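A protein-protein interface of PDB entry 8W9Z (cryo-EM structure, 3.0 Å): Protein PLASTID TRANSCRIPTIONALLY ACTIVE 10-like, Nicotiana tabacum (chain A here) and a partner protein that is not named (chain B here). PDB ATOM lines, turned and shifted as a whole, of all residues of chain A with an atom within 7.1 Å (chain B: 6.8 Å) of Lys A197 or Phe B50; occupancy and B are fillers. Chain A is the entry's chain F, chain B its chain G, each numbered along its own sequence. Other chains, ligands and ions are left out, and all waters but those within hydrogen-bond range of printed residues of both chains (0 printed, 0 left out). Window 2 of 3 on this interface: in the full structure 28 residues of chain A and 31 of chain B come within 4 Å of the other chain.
OD1 of Asn B90 sits close to O of Ala B51.
The backbone carbonyl oxygen (O) of Phe B50 lies close to the side-chain hydroxyl (OH) of Tyr B100 (3.3 Å).
OG of Ser A200 sits at hydrogen-bond distance from O of Lys A197 (3.0 Å).
The side-chain hydroxyl (OH) of Tyr B100 lies close to the backbone NH (N) of Ala B51, 3.4 Å away.
N of Val B49 lies close to OE1 of Glu A190 (3.4 Å).
NH1 of Arg A175 sits at hydrogen-bond distance from OH of Tyr B52.
O of Tyr B100 sits at hydrogen-bond distance from NH2 of Arg A175.
Among the printed residues, merely in contact across the chains: His A196 with Tyr B100 (3.2 Å), Lys A197 with Phe B50 (3.3 Å), Ser A200 with Gly B54 (3.3 Å), Lys A197 with Tyr B53 (3.3 Å), Arg A175 with Ala B51 (3.4 Å), Arg A193 with Val B49 (3.4 Å), Arg A193 with Tyr B100 (3.5 Å) and Arg A193 with Phe B50 (3.9 Å).
Printed residues of chain A that touch a printed residue of chain B: Arg A175, Glu A190, Arg A193, His A196, Lys A197 and Ser A200.
Hydrophobic or aromatic side chains of chain A within 4 Å of the printed part of chain B: His A196.
Printed residues of chain B that touch a printed residue of chain A: Val B49, Phe B50, Ala B51, Tyr B52, Tyr B53, Gly B54 and Tyr B100.
Along chain B the printed residues that touch a printed residue of chain A span positions 49 to 100.
Among the printed residues, 11 pairs touch across the chains.
Among the printed residues, no Asp or Glu carboxylate lies within 4 Å of a Lys or Arg side-chain nitrogen of the other chain.
Printed residues of chain B within 4 Å of Glu A190: Val B49.
Lys A197 touches just these residues of chain B: Phe B50 (3.3 Å) and Tyr B53 (3.3 Å).
Printed residues of chain B within 4 Å of Ser A200: Gly B54 (3.3 Å).
Phe B50 touches just these residues of chain A: Arg A193 and Lys A197.
Printed residues of chain A within 4 Å of Tyr B52: Arg A175 (3.0 Å).
Printed residues of chain A within 4 Å of Gly B54: Ser A200 (3.3 Å).
Leu B93 touches none of the printed residues of chain A.
Glu B94 touches none of the printed residues of chain A.
Of the printed residues of chain A, Tyr B100 touches Arg A175, Arg A193 and His A196.
The nearest residue of chain A that does not touch Phe B50 is His A196 (4.1 Å).
The nearest printed residue of chain B that does not touch Ser A200 is Tyr B53 (4.2 Å).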
ATOM      1  N   ARG A 170       5.301  21.208 -19.778  1.00  0.00           N
ATOM      2  CA  ARG A 170       5.786  20.396 -20.887  1.00  0.00           C
ATOM      3  C   ARG A 170       7.033  19.653 -20.433  1.00  0.00           C
ATOM      4  O   ARG A 170       7.932  20.255 -19.839  1.00  0.00           O
ATOM      5  CB  ARG A 170       6.096  21.260 -22.114  1.00  0.00           C
ATOM      6  CG  ARG A 170       6.635  20.481 -23.302  1.00  0.00           C
ATOM      7  CD  ARG A 170       6.771  21.367 -24.530  1.00  0.00           C
ATOM      8  NE  ARG A 170       7.781  22.405 -24.349  1.00  0.00           N
ATOM      9  CZ  ARG A 170       9.056  22.271 -24.697  1.00  0.00           C
ATOM     10  NH1 ARG A 170       9.908  23.267 -24.495  1.00  0.00           N
ATOM     11  NH2 ARG A 170       9.480  21.143 -25.247  1.00  0.00           N
ATOM     12  N   ARG A 175      19.005  19.886 -19.362  1.00  0.00           N
ATOM     13  CA  ARG A 175      20.066  20.423 -20.208  1.00  0.00           C
ATOM     14  C   ARG A 175      21.402  19.760 -19.904  1.00  0.00           C
ATOM     15  O   ARG A 175      22.246  19.615 -20.795  1.00  0.00           O
ATOM     16  CB  ARG A 175      20.164  21.936 -20.029  1.00  0.00           C
ATOM     17  CG  ARG A 175      18.923  22.698 -20.455  1.00  0.00           C
ATOM     18  CD  ARG A 175      19.105  24.185 -20.222  1.00  0.00           C
ATOM     19  NE  ARG A 175      20.225  24.720 -20.988  1.00  0.00           N
ATOM     20  CZ  ARG A 175      20.862  25.845 -20.683  1.00  0.00           C
ATOM     21  NH1 ARG A 175      20.495  26.545 -19.619  1.00  0.00           N
ATOM     22  NH2 ARG A 175      21.873  26.264 -21.432  1.00  0.00           N
ATOM     23  N   GLU A 190      21.709  15.280 -30.301  1.00  0.00           N
ATOM     24  CA  GLU A 190      21.284  16.462 -31.044  1.00  0.00           C
ATOM     25  C   GLU A 190      19.765  16.543 -31.120  1.00  0.00           C
ATOM     26  O   GLU A 190      19.173  17.601 -30.869  1.00  0.00           O
ATOM     27  CB  GLU A 190      21.890  16.442 -32.447  1.00  0.00           C
ATOM     28  CG  GLU A 190      23.374  16.753 -32.488  1.00  0.00           C
ATOM     29  CD  GLU A 190      23.658  18.220 -32.264  1.00  0.00           C
ATOM     30  OE1 GLU A 190      22.741  19.037 -32.492  1.00  0.00           O
ATOM     31  OE2 GLU A 190      24.791  18.554 -31.860  1.00  0.00           O
ATOM     32  N   ARG A 193      18.504  17.558 -27.633  1.00  0.00           N
ATOM     33  CA  ARG A 193      18.732  18.967 -27.338  1.00  0.00           C
ATOM     34  C   ARG A 193      17.947  19.900 -28.249  1.00  0.00           C
ATOM     35  O   ARG A 193      17.842  21.091 -27.939  1.00  0.00           O
ATOM     36  CB  ARG A 193      20.223  19.293 -27.442  1.00  0.00           C
ATOM     37  CG  ARG A 193      21.079  18.654 -26.366  1.00  0.00           C
ATOM     38  CD  ARG A 193      22.537  19.043 -26.528  1.00  0.00           C
ATOM     39  NE  ARG A 193      23.371  18.497 -25.463  1.00  0.00           N
ATOM     40  CZ  ARG A 193      24.688  18.660 -25.390  1.00  0.00           C
ATOM     41  NH1 ARG A 193      25.324  19.355 -26.323  1.00  0.00           N
ATOM     42  NH2 ARG A 193      25.369  18.130 -24.385  1.00  0.00           N
ATOM     43  N   GLU A 194      17.411  19.395 -29.362  1.00  0.00           N
ATOM     44  CA  GLU A 194      16.591  20.231 -30.233  1.00  0.00           C
ATOM     45  C   GLU A 194      15.384  20.811 -29.502  1.00  0.00           C
ATOM     46  O   GLU A 194      14.884  21.877 -29.881  1.00  0.00           O
ATOM     47  CB  GLU A 194      16.140  19.424 -31.452  1.00  0.00           C
ATOM     48  CG  GLU A 194      15.380  20.224 -32.501  1.00  0.00           C
ATOM     49  CD  GLU A 194      16.252  21.239 -33.215  1.00  0.00           C
ATOM     50  OE1 GLU A 194      17.490  21.076 -33.208  1.00  0.00           O
ATOM     51  OE2 GLU A 194      15.697  22.201 -33.785  1.00  0.00           O
ATOM     52  N   THR A 195      14.909  20.139 -28.449  1.00  0.00           N
ATOM     53  CA  THR A 195      13.708  20.597 -27.757  1.00  0.00           C
ATOM     54  C   THR A 195      13.939  21.871 -26.955  1.00  0.00           C
ATOM     55  O   THR A 195      12.964  22.532 -26.579  1.00  0.00           O
ATOM     56  CB  THR A 195      13.175  19.504 -26.829  1.00  0.00           C
ATOM     57  OG1 THR A 195      11.862  19.859 -26.380  1.00  0.00           O
ATOM     58  CG2 THR A 195      14.080  19.347 -25.620  1.00  0.00           C
ATOM     59  N   HIS A 196      15.195  22.231 -26.680  1.00  0.00           N
ATOM     60  CA  HIS A 196      15.459  23.442 -25.912  1.00  0.00           C
ATOM     61  C   HIS A 196      15.124  24.697 -26.707  1.00  0.00           C
ATOM     62  O   HIS A 196      14.842  25.745 -26.118  1.00  0.00           O
ATOM     63  CB  HIS A 196      16.918  23.468 -25.462  1.00  0.00           C
ATOM     64  CG  HIS A 196      17.307  22.302 -24.609  1.00  0.00           C
ATOM     65  ND1 HIS A 196      16.424  21.676 -23.758  1.00  0.00           N
ATOM     66  CD2 HIS A 196      18.485  21.645 -24.479  1.00  0.00           C
ATOM     67  CE1 HIS A 196      17.040  20.685 -23.138  1.00  0.00           C
ATOM     68  NE2 HIS A 196      18.291  20.644 -23.558  1.00  0.00           N
ATOM     69  N   LYS A 197      15.151  24.612 -28.039  1.00  0.00           N
ATOM     70  CA  LYS A 197      14.798  25.764 -28.862  1.00  0.00           C
ATOM     71  C   LYS A 197      13.313  26.080 -28.760  1.00  0.00           C
ATOM     72  O   LYS A 197      12.917  27.252 -28.786  1.00  0.00           O
ATOM     73  CB  LYS A 197      15.184  25.505 -30.318  1.00  0.00           C
ATOM     74  CG  LYS A 197      16.645  25.152 -30.536  1.00  0.00           C
ATOM     75  CD  LYS A 197      16.888  24.733 -31.977  1.00  0.00           C
ATOM     76  CE  LYS A 197      18.363  24.496 -32.252  1.00  0.00           C
ATOM     77  NZ  LYS A 197      19.143  25.762 -32.208  1.00  0.00           N
ATOM     78  N   LEU A 198      12.475  25.049 -28.641  1.00  0.00           N
ATOM     79  CA  LEU A 198      11.029  25.232 -28.626  1.00  0.00           C
ATOM     80  C   LEU A 198      10.516  25.826 -27.321  1.00  0.00           C
ATOM     81  O   LEU A 198       9.345  26.215 -27.260  1.00  0.00           O
ATOM     82  CB  LEU A 198      10.334  23.895 -28.890  1.00  0.00           C
ATOM     83  CG  LEU A 198      10.747  23.165 -30.168  1.00  0.00           C
ATOM     84  CD1 LEU A 198      10.009  21.841 -30.293  1.00  0.00           C
ATOM     85  CD2 LEU A 198      10.499  24.038 -31.389  1.00  0.00           C
ATOM     86  N   GLN A 199      11.350  25.905 -26.285  1.00  0.00           N
ATOM     87  CA  GLN A 199      10.907  26.444 -25.006  1.00  0.00           C
ATOM     88  C   GLN A 199      10.773  27.961 -25.024  1.00  0.00           C
ATOM     89  O   GLN A 199      10.131  28.524 -24.131  1.00  0.00           O
ATOM     90  CB  GLN A 199      11.875  26.018 -23.897  1.00  0.00           C
ATOM     91  CG  GLN A 199      11.297  26.101 -22.493  1.00  0.00           C
ATOM     92  CD  GLN A 199      12.267  25.615 -21.435  1.00  0.00           C
ATOM     93  OE1 GLN A 199      13.395  25.228 -21.742  1.00  0.00           O
ATOM     94  NE2 GLN A 199      11.832  25.633 -20.181  1.00  0.00           N
ATOM     95  N   SER A 200      11.353  28.631 -26.019  1.00  0.00           N
ATOM     96  CA  SER A 200      11.297  30.086 -26.086  1.00  0.00           C
ATOM     97  C   SER A 200       9.955  30.607 -26.580  1.00  0.00           C
ATOM     98  O   SER A 200       9.669  31.797 -26.408  1.00  0.00           O
ATOM     99  CB  SER A 200      12.413  30.614 -26.989  1.00  0.00           C
ATOM    100  OG  SER A 200      12.283  30.108 -28.307  1.00  0.00           O
ATOM    101  N   VAL A 201       9.131  29.755 -27.191  1.00  0.00           N
ATOM    102  CA  VAL A 201       7.839  30.204 -27.693  1.00  0.00           C
ATOM    103  C   VAL A 201       6.903  30.487 -26.522  1.00  0.00           C
ATOM    104  O   VAL A 201       7.028  29.904 -25.436  1.00  0.00           O
ATOM    105  CB  VAL A 201       7.239  29.163 -28.657  1.00  0.00           C
ATOM    106  CG1 VAL A 201       6.694  27.964 -27.893  1.00  0.00           C
ATOM    107  CG2 VAL A 201       6.159  29.793 -29.531  1.00  0.00           C
ATOM    108  N   VAL B  49      22.414  20.754 -29.602  1.00  0.00           N
ATOM    109  CA  VAL B  49      23.632  21.528 -29.802  1.00  0.00           C
ATOM    110  C   VAL B  49      23.495  22.907 -29.181  1.00  0.00           C
ATOM    111  O   VAL B  49      24.433  23.424 -28.576  1.00  0.00           O
ATOM    112  CB  VAL B  49      23.977  21.653 -31.295  1.00  0.00           C
ATOM    113  N   PHE B  50      22.316  23.501 -29.335  1.00  0.00           N
ATOM    114  CA  PHE B  50      22.069  24.875 -28.926  1.00  0.00           C
ATOM    115  C   PHE B  50      20.942  24.920 -27.908  1.00  0.00           C
ATOM    116  O   PHE B  50      19.861  24.369 -28.145  1.00  0.00           O
ATOM    117  CB  PHE B  50      21.721  25.749 -30.134  1.00  0.00           C
ATOM    118  N   ALA B  51      21.198  25.575 -26.781  1.00  0.00           N
ATOM    119  CA  ALA B  51      20.183  25.870 -25.784  1.00  0.00           C
ATOM    120  C   ALA B  51      19.950  27.373 -25.752  1.00  0.00           C
ATOM    121  O   ALA B  51      20.790  28.159 -26.197  1.00  0.00           O
ATOM    122  CB  ALA B  51      20.591  25.365 -24.395  1.00  0.00           C
ATOM    123  N   TYR B  52      18.789  27.764 -25.223  1.00  0.00           N
ATOM    124  CA  TYR B  52      18.357  29.161 -25.219  1.00  0.00           C
ATOM    125  C   TYR B  52      18.289  29.728 -26.634  1.00  0.00           C
ATOM    126  O   TYR B  52      18.385  30.941 -26.834  1.00  0.00           O
ATOM    127  CB  TYR B  52      19.265  30.026 -24.341  1.00  0.00           C
ATOM    128  CG  TYR B  52      19.156  29.730 -22.864  1.00  0.00           C
ATOM    129  CD1 TYR B  52      17.936  29.394 -22.293  1.00  0.00           C
ATOM    130  CD2 TYR B  52      20.272  29.785 -22.041  1.00  0.00           C
ATOM    131  CE1 TYR B  52      17.831  29.124 -20.942  1.00  0.00           C
ATOM    132  CE2 TYR B  52      20.177  29.519 -20.691  1.00  0.00           C
ATOM    133  CZ  TYR B  52      18.955  29.188 -20.146  1.00  0.00           C
ATOM    134  OH  TYR B  52      18.857  28.918 -18.800  1.00  0.00           O
ATOM    135  N   TYR B  53      18.119  28.852 -27.624  1.00  0.00           N
ATOM    136  CA  TYR B  53      18.112  29.252 -29.031  1.00  0.00           C
ATOM    137  C   TYR B  53      16.707  29.723 -29.394  1.00  0.00           C
ATOM    138  O   TYR B  53      15.920  29.023 -30.033  1.00  0.00           O
ATOM    139  CB  TYR B  53      18.574  28.105 -29.918  1.00  0.00           C
ATOM    140  N   GLY B  54      16.398  30.943 -28.970  1.00  0.00           N
ATOM    141  CA  GLY B  54      15.118  31.548 -29.268  1.00  0.00           C
ATOM    142  C   GLY B  54      15.101  33.024 -28.935  1.00  0.00           C
ATOM    143  O   GLY B  54      15.537  33.425 -27.852  1.00  0.00           O
ATOM    144  N   GLU B  87      22.561  33.705 -31.545  1.00  0.00           N
ATOM    145  CA  GLU B  87      23.308  32.825 -32.441  1.00  0.00           C
ATOM    146  C   GLU B  87      24.728  32.597 -31.935  1.00  0.00           C
ATOM    147  O   GLU B  87      25.217  31.460 -31.910  1.00  0.00           O
ATOM    148  CB  GLU B  87      23.324  33.407 -33.855  1.00  0.00           C
ATOM    149  CG  GLU B  87      21.974  33.386 -34.554  1.00  0.00           C
ATOM    150  CD  GLU B  87      21.501  31.981 -34.876  1.00  0.00           C
ATOM    151  OE1 GLU B  87      22.349  31.069 -34.969  1.00  0.00           O
ATOM    152  OE2 GLU B  87      20.277  31.789 -35.038  1.00  0.00           O
ATOM    153  N   LEU B  89      25.796  32.967 -28.842  1.00  0.00           N
ATOM    154  CA  LEU B  89      25.732  32.205 -27.599  1.00  0.00           C
ATOM    155  C   LEU B  89      25.545  30.721 -27.876  1.00  0.00           C
ATOM    156  O   LEU B  89      26.145  29.876 -27.203  1.00  0.00           O
ATOM    157  CB  LEU B  89      24.604  32.736 -26.716  1.00  0.00           C
ATOM    158  CG  LEU B  89      24.417  32.036 -25.370  1.00  0.00           C
ATOM    159  CD1 LEU B  89      25.691  32.109 -24.547  1.00  0.00           C
ATOM    160  CD2 LEU B  89      23.249  32.642 -24.610  1.00  0.00           C
ATOM    161  N   ASN B  90      24.724  30.383 -28.872  1.00  0.00           N
ATOM    162  CA  ASN B  90      24.566  28.982 -29.251  1.00  0.00           C
ATOM    163  C   ASN B  90      25.868  28.411 -29.797  1.00  0.00           C
ATOM    164  O   ASN B  90      26.248  27.279 -29.469  1.00  0.00           O
ATOM    165  CB  ASN B  90      23.449  28.843 -30.284  1.00  0.00           C
ATOM    166  CG  ASN B  90      22.107  29.300 -29.755  1.00  0.00           C
ATOM    167  OD1 ASN B  90      21.822  29.176 -28.566  1.00  0.00           O
ATOM    168  ND2 ASN B  90      21.274  29.836 -30.638  1.00  0.00           N
ATOM    169  N   LYS B  91      26.562  29.180 -30.640  1.00  0.00           N
ATOM    170  CA  LYS B  91      27.833  28.715 -31.188  1.00  0.00           C
ATOM    171  C   LYS B  91      28.873  28.507 -30.096  1.00  0.00           C
ATOM    172  O   LYS B  91      29.702  27.596 -30.195  1.00  0.00           O
ATOM    173  CB  LYS B  91      28.350  29.704 -32.233  1.00  0.00           C
ATOM    174  CG  LYS B  91      27.497  29.785 -33.487  1.00  0.00           C
ATOM    175  CD  LYS B  91      27.421  28.440 -34.191  1.00  0.00           C
ATOM    176  CE  LYS B  91      26.561  28.519 -35.442  1.00  0.00           C
ATOM    177  NZ  LYS B  91      25.164  28.933 -35.131  1.00  0.00           N
ATOM    178  N   LEU B  93      28.094  27.786 -26.849  1.00  0.00           N
ATOM    179  CA  LEU B  93      27.647  26.690 -25.997  1.00  0.00           C
ATOM    180  C   LEU B  93      27.837  25.334 -26.662  1.00  0.00           C
ATOM    181  O   LEU B  93      27.977  24.324 -25.964  1.00  0.00           O
ATOM    182  CB  LEU B  93      26.177  26.876 -25.615  1.00  0.00           C
ATOM    183  CG  LEU B  93      25.864  27.943 -24.566  1.00  0.00           C
ATOM    184  CD1 LEU B  93      24.366  28.035 -24.332  1.00  0.00           C
ATOM    185  CD2 LEU B  93      26.594  27.642 -23.268  1.00  0.00           C
ATOM    186  N   GLU B  94      27.830  25.287 -27.996  1.00  0.00           N
ATOM    187  CA  GLU B  94      28.096  24.025 -28.681  1.00  0.00           C
ATOM    188  C   GLU B  94      29.500  23.512 -28.387  1.00  0.00           C
ATOM    189  O   GLU B  94      29.707  22.298 -28.271  1.00  0.00           O
ATOM    190  CB  GLU B  94      27.885  24.194 -30.188  1.00  0.00           C
ATOM    191  CG  GLU B  94      28.596  23.164 -31.062  1.00  0.00           C
ATOM    192  CD  GLU B  94      28.096  21.745 -30.851  1.00  0.00           C
ATOM    193  OE1 GLU B  94      27.003  21.567 -30.276  1.00  0.00           O
ATOM    194  OE2 GLU B  94      28.802  20.801 -31.265  1.00  0.00           O
ATOM    195  N   TYR B 100      27.003  24.214 -20.921  1.00  0.00           N
ATOM    196  CA  TYR B 100      25.733  24.043 -21.618  1.00  0.00           C
ATOM    197  C   TYR B 100      24.622  23.673 -20.645  1.00  0.00           C
ATOM    198  O   TYR B 100      23.517  24.223 -20.708  1.00  0.00           O
ATOM    199  CB  TYR B 100      25.875  22.980 -22.707  1.00  0.00           C
ATOM    200  CG  TYR B 100      24.642  22.799 -23.563  1.00  0.00           C
ATOM    201  CD1 TYR B 100      24.456  23.556 -24.709  1.00  0.00           C
ATOM    202  CD2 TYR B 100      23.670  21.868 -23.228  1.00  0.00           C
ATOM    203  CE1 TYR B 100      23.333  23.394 -25.496  1.00  0.00           C
ATOM    204  CE2 TYR B 100      22.545  21.700 -24.007  1.00  0.00           C
ATOM    205  CZ  TYR B 100      22.381  22.464 -25.141  1.00  0.00           C
ATOM    206  OH  TYR B 100      21.260  22.298 -25.920  1.00  0.00           O
